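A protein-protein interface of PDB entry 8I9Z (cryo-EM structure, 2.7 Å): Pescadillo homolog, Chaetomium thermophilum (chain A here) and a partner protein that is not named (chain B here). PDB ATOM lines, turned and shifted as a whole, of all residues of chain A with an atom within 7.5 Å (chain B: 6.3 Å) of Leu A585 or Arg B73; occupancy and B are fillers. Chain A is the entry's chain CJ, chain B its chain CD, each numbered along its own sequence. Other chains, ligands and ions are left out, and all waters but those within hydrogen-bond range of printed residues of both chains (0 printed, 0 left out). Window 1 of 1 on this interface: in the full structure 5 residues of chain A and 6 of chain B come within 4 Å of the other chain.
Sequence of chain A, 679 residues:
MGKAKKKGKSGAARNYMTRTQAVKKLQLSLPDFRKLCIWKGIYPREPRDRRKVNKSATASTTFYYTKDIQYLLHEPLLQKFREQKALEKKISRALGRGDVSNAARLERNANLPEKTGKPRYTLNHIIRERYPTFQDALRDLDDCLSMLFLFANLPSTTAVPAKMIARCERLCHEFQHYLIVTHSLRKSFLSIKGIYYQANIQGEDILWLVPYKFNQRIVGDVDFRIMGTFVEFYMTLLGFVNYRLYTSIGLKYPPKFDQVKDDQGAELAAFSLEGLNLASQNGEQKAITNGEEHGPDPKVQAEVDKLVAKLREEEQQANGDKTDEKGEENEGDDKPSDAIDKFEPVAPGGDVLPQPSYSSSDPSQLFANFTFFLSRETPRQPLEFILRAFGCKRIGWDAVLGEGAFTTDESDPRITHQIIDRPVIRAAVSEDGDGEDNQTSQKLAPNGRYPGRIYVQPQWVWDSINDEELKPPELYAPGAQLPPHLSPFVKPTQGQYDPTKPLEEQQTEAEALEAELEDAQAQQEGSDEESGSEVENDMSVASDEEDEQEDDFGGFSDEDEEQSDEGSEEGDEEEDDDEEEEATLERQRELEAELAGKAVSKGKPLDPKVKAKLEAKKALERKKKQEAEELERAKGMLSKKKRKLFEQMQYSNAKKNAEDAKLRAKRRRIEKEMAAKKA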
ATOM      1  N   GLU A 582     -11.676  -7.161 -20.455  1.00  0.00           N
ATOM      2  CA  GLU A 582     -11.281  -5.859 -20.979  1.00  0.00           C
ATOM      3  C   GLU A 582     -11.853  -4.728 -20.132  1.00  0.00           C
ATOM      4  O   GLU A 582     -11.162  -3.751 -19.842  1.00  0.00           O
ATOM      5  CB  GLU A 582     -11.731  -5.706 -22.433  1.00  0.00           C
ATOM      6  CG  GLU A 582     -11.009  -6.624 -23.407  1.00  0.00           C
ATOM      7  CD  GLU A 582     -11.566  -6.535 -24.814  1.00  0.00           C
ATOM      8  OE1 GLU A 582     -12.625  -5.898 -24.997  1.00  0.00           O
ATOM      9  OE2 GLU A 582     -10.945  -7.103 -25.738  1.00  0.00           O
ATOM     10  N   ALA A 583     -13.125  -4.868 -19.748  1.00  0.00           N
ATOM     11  CA  ALA A 583     -13.782  -3.833 -18.954  1.00  0.00           C
ATOM     12  C   ALA A 583     -13.186  -3.738 -17.555  1.00  0.00           C
ATOM     13  O   ALA A 583     -12.940  -2.634 -17.055  1.00  0.00           O
ATOM     14  CB  ALA A 583     -15.284  -4.104 -18.882  1.00  0.00           C
ATOM     15  N   THR A 584     -12.943  -4.883 -16.912  1.00  0.00           N
ATOM     16  CA  THR A 584     -12.327  -4.870 -15.588  1.00  0.00           C
ATOM     17  C   THR A 584     -10.877  -4.413 -15.665  1.00  0.00           C
ATOM     18  O   THR A 584     -10.341  -3.851 -14.702  1.00  0.00           O
ATOM     19  CB  THR A 584     -12.418  -6.256 -14.949  1.00  0.00           C
ATOM     20  OG1 THR A 584     -11.815  -7.223 -15.816  1.00  0.00           O
ATOM     21  CG2 THR A 584     -13.871  -6.636 -14.713  1.00  0.00           C
ATOM     22  N   LEU A 585     -10.224  -4.648 -16.806  1.00  0.00           N
ATOM     23  CA  LEU A 585      -8.866  -4.152 -16.992  1.00  0.00           C
ATOM     24  C   LEU A 585      -8.848  -2.640 -17.150  1.00  0.00           C
ATOM     25  O   LEU A 585      -7.908  -1.976 -16.699  1.00  0.00           O
ATOM     26  CB  LEU A 585      -8.217  -4.822 -18.202  1.00  0.00           C
ATOM     27  CG  LEU A 585      -8.462  -6.316 -18.413  1.00  0.00           C
ATOM     28  CD1 LEU A 585      -7.861  -6.762 -19.736  1.00  0.00           C
ATOM     29  CD2 LEU A 585      -7.892  -7.127 -17.259  1.00  0.00           C
ATOM     30  N   GLU A 586      -9.878  -2.079 -17.786  1.00  0.00           N
ATOM     31  CA  GLU A 586      -9.937  -0.635 -17.992  1.00  0.00           C
ATOM     32  C   GLU A 586     -10.057   0.105 -16.667  1.00  0.00           C
ATOM     33  O   GLU A 586      -9.483   1.185 -16.494  1.00  0.00           O
ATOM     34  CB  GLU A 586     -11.104  -0.277 -18.914  1.00  0.00           C
ATOM     35  CG  GLU A 586     -10.840  -0.524 -20.390  1.00  0.00           C
ATOM     36  CD  GLU A 586     -12.109  -0.513 -21.218  1.00  0.00           C
ATOM     37  OE1 GLU A 586     -13.208  -0.518 -20.623  1.00  0.00           O
ATOM     38  OE2 GLU A 586     -12.011  -0.499 -22.463  1.00  0.00           O
ATOM     39  N   ARG A 587     -10.805  -0.462 -15.719  1.00  0.00           N
ATOM     40  CA  ARG A 587     -10.879   0.133 -14.389  1.00  0.00           C
ATOM     41  C   ARG A 587      -9.552   0.004 -13.652  1.00  0.00           C
ATOM     42  O   ARG A 587      -9.238   0.820 -12.780  1.00  0.00           O
ATOM     43  CB  ARG A 587     -12.006  -0.509 -13.583  1.00  0.00           C
ATOM     44  CG  ARG A 587     -13.306   0.284 -13.606  1.00  0.00           C
ATOM     45  CD  ARG A 587     -14.218  -0.134 -14.749  1.00  0.00           C
ATOM     46  NE  ARG A 587     -14.772  -1.467 -14.546  1.00  0.00           N
ATOM     47  CZ  ARG A 587     -15.531  -2.104 -15.427  1.00  0.00           C
ATOM     48  NH1 ARG A 587     -15.850  -1.556 -16.588  1.00  0.00           N
ATOM     49  NH2 ARG A 587     -15.981  -3.322 -15.136  1.00  0.00           N
ATOM     50  N   GLN A 588      -8.762  -1.018 -13.986  1.00  0.00           N
ATOM     51  CA  GLN A 588      -7.481  -1.213 -13.314  1.00  0.00           C
ATOM     52  C   GLN A 588      -6.463  -0.162 -13.745  1.00  0.00           C
ATOM     53  O   GLN A 588      -5.732   0.387 -12.912  1.00  0.00           O
ATOM     54  CB  GLN A 588      -6.961  -2.623 -13.584  1.00  0.00           C
ATOM     55  CG  GLN A 588      -7.574  -3.676 -12.672  1.00  0.00           C
ATOM     56  CD  GLN A 588      -7.119  -5.080 -13.009  1.00  0.00           C
ATOM     57  OE1 GLN A 588      -6.768  -5.372 -14.152  1.00  0.00           O
ATOM     58  NE2 GLN A 588      -7.128  -5.961 -12.015  1.00  0.00           N
ATOM     59  N   ARG A 589      -6.404   0.139 -15.044  1.00  0.00           N
ATOM     60  CA  ARG A 589      -5.474   1.164 -15.512  1.00  0.00           C
ATOM     61  C   ARG A 589      -5.958   2.559 -15.146  1.00  0.00           C
ATOM     62  O   ARG A 589      -5.150   3.484 -14.997  1.00  0.00           O
ATOM     63  CB  ARG A 589      -5.253   1.053 -17.022  1.00  0.00           C
ATOM     64  CG  ARG A 589      -5.272  -0.356 -17.589  1.00  0.00           C
ATOM     65  CD  ARG A 589      -4.139  -1.195 -17.023  1.00  0.00           C
ATOM     66  NE  ARG A 589      -2.875  -0.902 -17.685  1.00  0.00           N
ATOM     67  CZ  ARG A 589      -2.066  -1.820 -18.195  1.00  0.00           C
ATOM     68  NH1 ARG A 589      -2.358  -3.109 -18.132  1.00  0.00           N
ATOM     69  NH2 ARG A 589      -0.934  -1.436 -18.777  1.00  0.00           N
ATOM     70  N   GLU A 590      -7.270   2.736 -15.000  1.00  0.00           N
ATOM     71  CA  GLU A 590      -7.787   4.028 -14.564  1.00  0.00           C
ATOM     72  C   GLU A 590      -7.482   4.270 -13.092  1.00  0.00           C
ATOM     73  O   GLU A 590      -7.154   5.396 -12.695  1.00  0.00           O
ATOM     74  CB  GLU A 590      -9.290   4.107 -14.825  1.00  0.00           C
ATOM     75  CG  GLU A 590      -9.656   4.449 -16.261  1.00  0.00           C
ATOM     76  CD  GLU A 590     -11.154   4.514 -16.477  1.00  0.00           C
ATOM     77  OE1 GLU A 590     -11.905   4.068 -15.585  1.00  0.00           O
ATOM     78  OE2 GLU A 590     -11.581   5.015 -17.538  1.00  0.00           O
ATOM     79  N   LEU A 591      -7.573   3.224 -12.269  1.00  0.00           N
ATOM     80  CA  LEU A 591      -7.344   3.386 -10.836  1.00  0.00           C
ATOM     81  C   LEU A 591      -5.875   3.640 -10.532  1.00  0.00           C
ATOM     82  O   LEU A 591      -5.549   4.328  -9.558  1.00  0.00           O
ATOM     83  CB  LEU A 591      -7.847   2.162 -10.072  1.00  0.00           C
ATOM     84  CG  LEU A 591      -9.340   2.138  -9.736  1.00  0.00           C
ATOM     85  CD1 LEU A 591      -9.704   0.865  -8.982  1.00  0.00           C
ATOM     86  CD2 LEU A 591      -9.738   3.379  -8.942  1.00  0.00           C
ATOM     87  N   ARG B  42       0.786  -7.149  -7.860  1.00  0.00           N
ATOM     88  CA  ARG B  42       0.469  -6.647  -9.191  1.00  0.00           C
ATOM     89  C   ARG B  42       1.451  -5.548  -9.588  1.00  0.00           C
ATOM     90  O   ARG B  42       2.391  -5.230  -8.856  1.00  0.00           O
ATOM     91  CB  ARG B  42      -0.974  -6.136  -9.252  1.00  0.00           C
ATOM     92  CG  ARG B  42      -2.003  -7.115  -8.714  1.00  0.00           C
ATOM     93  CD  ARG B  42      -3.394  -6.792  -9.238  1.00  0.00           C
ATOM     94  NE  ARG B  42      -3.383  -6.426 -10.650  1.00  0.00           N
ATOM     95  CZ  ARG B  42      -3.370  -7.289 -11.657  1.00  0.00           C
ATOM     96  NH1 ARG B  42      -3.363  -8.596 -11.448  1.00  0.00           N
ATOM     97  NH2 ARG B  42      -3.364  -6.831 -12.905  1.00  0.00           N
ATOM     98  N   PHE B  65       6.056  -2.753 -17.643  1.00  0.00           N
ATOM     99  CA  PHE B  65       6.998  -3.864 -17.708  1.00  0.00           C
ATOM    100  C   PHE B  65       6.668  -4.791 -18.869  1.00  0.00           C
ATOM    101  O   PHE B  65       5.505  -4.914 -19.267  1.00  0.00           O
ATOM    102  CB  PHE B  65       7.076  -4.679 -16.408  1.00  0.00           C
ATOM    103  CG  PHE B  65       7.491  -3.908 -15.154  1.00  0.00           C
ATOM    104  CD1 PHE B  65       7.738  -4.622 -14.001  1.00  0.00           C
ATOM    105  CD2 PHE B  65       7.742  -2.538 -15.133  1.00  0.00           C
ATOM    106  CE1 PHE B  65       8.154  -3.999 -12.845  1.00  0.00           C
ATOM    107  CE2 PHE B  65       8.148  -1.909 -13.967  1.00  0.00           C
ATOM    108  CZ  PHE B  65       8.356  -2.645 -12.825  1.00  0.00           C
ATOM    109  N   ILE B  67       7.488  -8.733 -20.623  1.00  0.00           N
ATOM    110  CA  ILE B  67       8.011 -10.093 -20.547  1.00  0.00           C
ATOM    111  C   ILE B  67       7.741 -10.821 -21.862  1.00  0.00           C
ATOM    112  O   ILE B  67       6.625 -10.769 -22.389  1.00  0.00           O
ATOM    113  CB  ILE B  67       7.479 -10.867 -19.317  1.00  0.00           C
ATOM    114  CG1 ILE B  67       6.013 -10.549 -18.931  1.00  0.00           C
ATOM    115  CG2 ILE B  67       8.383 -10.650 -18.112  1.00  0.00           C
ATOM    116  CD1 ILE B  67       4.890 -10.987 -19.840  1.00  0.00           C
ATOM    117  N   PHE B  71       3.617  -6.976 -22.835  1.00  0.00           N
ATOM    118  CA  PHE B  71       3.531  -6.191 -21.617  1.00  0.00           C
ATOM    119  C   PHE B  71       2.945  -7.023 -20.480  1.00  0.00           C
ATOM    120  O   PHE B  71       2.429  -8.126 -20.673  1.00  0.00           O
ATOM    121  CB  PHE B  71       2.690  -4.936 -21.845  1.00  0.00           C
ATOM    122  CG  PHE B  71       3.497  -3.716 -22.176  1.00  0.00           C
ATOM    123  CD1 PHE B  71       4.858  -3.807 -22.418  1.00  0.00           C
ATOM    124  CD2 PHE B  71       2.891  -2.473 -22.246  1.00  0.00           C
ATOM    125  CE1 PHE B  71       5.600  -2.682 -22.722  1.00  0.00           C
ATOM    126  CE2 PHE B  71       3.625  -1.344 -22.550  1.00  0.00           C
ATOM    127  CZ  PHE B  71       4.983  -1.448 -22.789  1.00  0.00           C
ATOM    128  N   LEU B  72       3.039  -6.475 -19.274  1.00  0.00           N
ATOM    129  CA  LEU B  72       2.514  -7.119 -18.080  1.00  0.00           C
ATOM    130  C   LEU B  72       1.025  -6.813 -17.981  1.00  0.00           C
ATOM    131  O   LEU B  72       0.628  -5.645 -17.914  1.00  0.00           O
ATOM    132  CB  LEU B  72       3.273  -6.636 -16.842  1.00  0.00           C
ATOM    133  CG  LEU B  72       3.145  -7.345 -15.488  1.00  0.00           C
ATOM    134  CD1 LEU B  72       1.943  -6.872 -14.684  1.00  0.00           C
ATOM    135  CD2 LEU B  72       3.093  -8.853 -15.690  1.00  0.00           C
ATOM    136  N   ARG B  73       0.207  -7.861 -17.976  1.00  0.00           N
ATOM    137  CA  ARG B  73      -1.245  -7.741 -17.935  1.00  0.00           C
ATOM    138  C   ARG B  73      -1.846  -8.112 -16.592  1.00  0.00           C
ATOM    139  O   ARG B  73      -2.687  -7.377 -16.073  1.00  0.00           O
ATOM    140  CB  ARG B  73      -1.870  -8.616 -19.031  1.00  0.00           C
ATOM    141  CG  ARG B  73      -3.395  -8.712 -19.008  1.00  0.00           C
ATOM    142  CD  ARG B  73      -4.060  -7.377 -19.313  1.00  0.00           C
ATOM    143  NE  ARG B  73      -4.386  -6.639 -18.099  1.00  0.00           N
ATOM    144  CZ  ARG B  73      -4.739  -5.362 -18.068  1.00  0.00           C
ATOM    145  NH1 ARG B  73      -4.795  -4.634 -19.170  1.00  0.00           N
ATOM    146  NH2 ARG B  73      -5.043  -4.802 -16.901  1.00  0.00           N
ATOM    147  N   SER B  74      -1.422  -9.232 -16.011  1.00  0.00           N
ATOM    148  CA  SER B  74      -1.964  -9.709 -14.746  1.00  0.00           C
ATOM    149  C   SER B  74      -0.837  -9.966 -13.756  1.00  0.00           C
ATOM    150  O   SER B  74       0.312  -9.599 -14.015  1.00  0.00           O
ATOM    151  CB  SER B  74      -2.786 -10.978 -14.967  1.00  0.00           C
ATOM    152  OG  SER B  74      -1.943 -12.074 -15.277  1.00  0.00           O
ATOM    153  N   SER B  75      -1.149 -10.597 -12.627  1.00  0.00           N
ATOM    154  CA  SER B  75      -0.137 -10.876 -11.620  1.00  0.00           C
ATOM    155  C   SER B  75       0.852 -11.927 -12.120  1.00  0.00           C
ATOM    156  O   SER B  75       0.615 -12.625 -13.111  1.00  0.00           O
ATOM    157  CB  SER B  75      -0.785 -11.347 -10.319  1.00  0.00           C
ATOM    158  OG  SER B  75      -1.199 -12.697 -10.420  1.00  0.00           O
ATOM    159  N   GLU B 436      -2.829  -5.318 -27.475  1.00  0.00           N
ATOM    160  CA  GLU B 436      -4.037  -4.849 -26.825  1.00  0.00           C
ATOM    161  C   GLU B 436      -3.996  -3.342 -26.625  1.00  0.00           C
ATOM    162  O   GLU B 436      -2.943  -2.715 -26.772  1.00  0.00           O
ATOM    163  CB  GLU B 436      -4.221  -5.543 -25.469  1.00  0.00           C
ATOM    164  CG  GLU B 436      -4.094  -7.056 -25.530  1.00  0.00           C
ATOM    165  CD  GLU B 436      -5.039  -7.760 -24.575  1.00  0.00           C
ATOM    166  OE1 GLU B 436      -6.010  -7.121 -24.118  1.00  0.00           O
ATOM    167  OE2 GLU B 436      -4.810  -8.953 -24.286  1.00  0.00           O
ATOM    168  N   PRO B 437      -5.141  -2.722 -26.339  1.00  0.00           N
ATOM    169  CA  PRO B 437      -5.156  -1.295 -26.009  1.00  0.00           C
ATOM    170  C   PRO B 437      -4.319  -0.994 -24.775  1.00  0.00           C
ATOM    171  O   PRO B 437      -4.196  -1.817 -23.865  1.00  0.00           O
ATOM    172  CB  PRO B 437      -6.649  -1.030 -25.727  1.00  0.00           C
ATOM    173  CG  PRO B 437      -7.304  -2.445 -25.953  1.00  0.00           C
ATOM    174  CD  PRO B 437      -6.428  -2.990 -26.982  1.00  0.00           C
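The guanidinium group (NH1) of Arg B73 sits close to the guanidinium group (NH1) of Arg A589 (3.1 Å). NH2 of Arg B73 is in hydrogen-bond range of OE1 of Gln A588 (3.3 Å).
N of Leu B72 sits at hydrogen-bond distance from O of Phe B65, 2.9 Å away. O of Arg B73 is in hydrogen-bond range of NH2 of Arg B42 (3.3 Å).
Leu A585 touches Arg B73 (CB to NH2, 3.4 Å). OE1 of Gln A588 touches NH2 of Arg B42 (3.9 Å). Leu B72 touches Arg A589.
Arg A587 touches none of the printed residues of chain B. Printed residues of chain B within 4 Å of Gln A588: Arg B42 (3.9 Å) and Arg B73 (3.3 Å). Of the printed residues of chain B, Arg A589 touches Leu B72 and Arg B73. Printed residues of chain A within 4 Å of Arg B42: Gln A588. Of the printed residues of chain A, Leu B72 touches Arg A589 (3.9 Å). Arg B73 touches three residues of chain A. Ser B74 touches none of the printed residues of chain A. The nearest residue of chain B that does not touch Leu A585 is Glu B436 (4.8 Å). The nearest printed residue of chain B that does not touch Arg A589 is Phe B71 (5.3 Å).
Of the 10 printed residues of chain A, 3 touch a printed residue of chain B. Among the printed residues, 5 pairs touch across the chains. Among the printed residues, no Asp or Glu carboxylate lies within 4 Å of a Lys or Arg side-chain nitrogen of the other chain.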
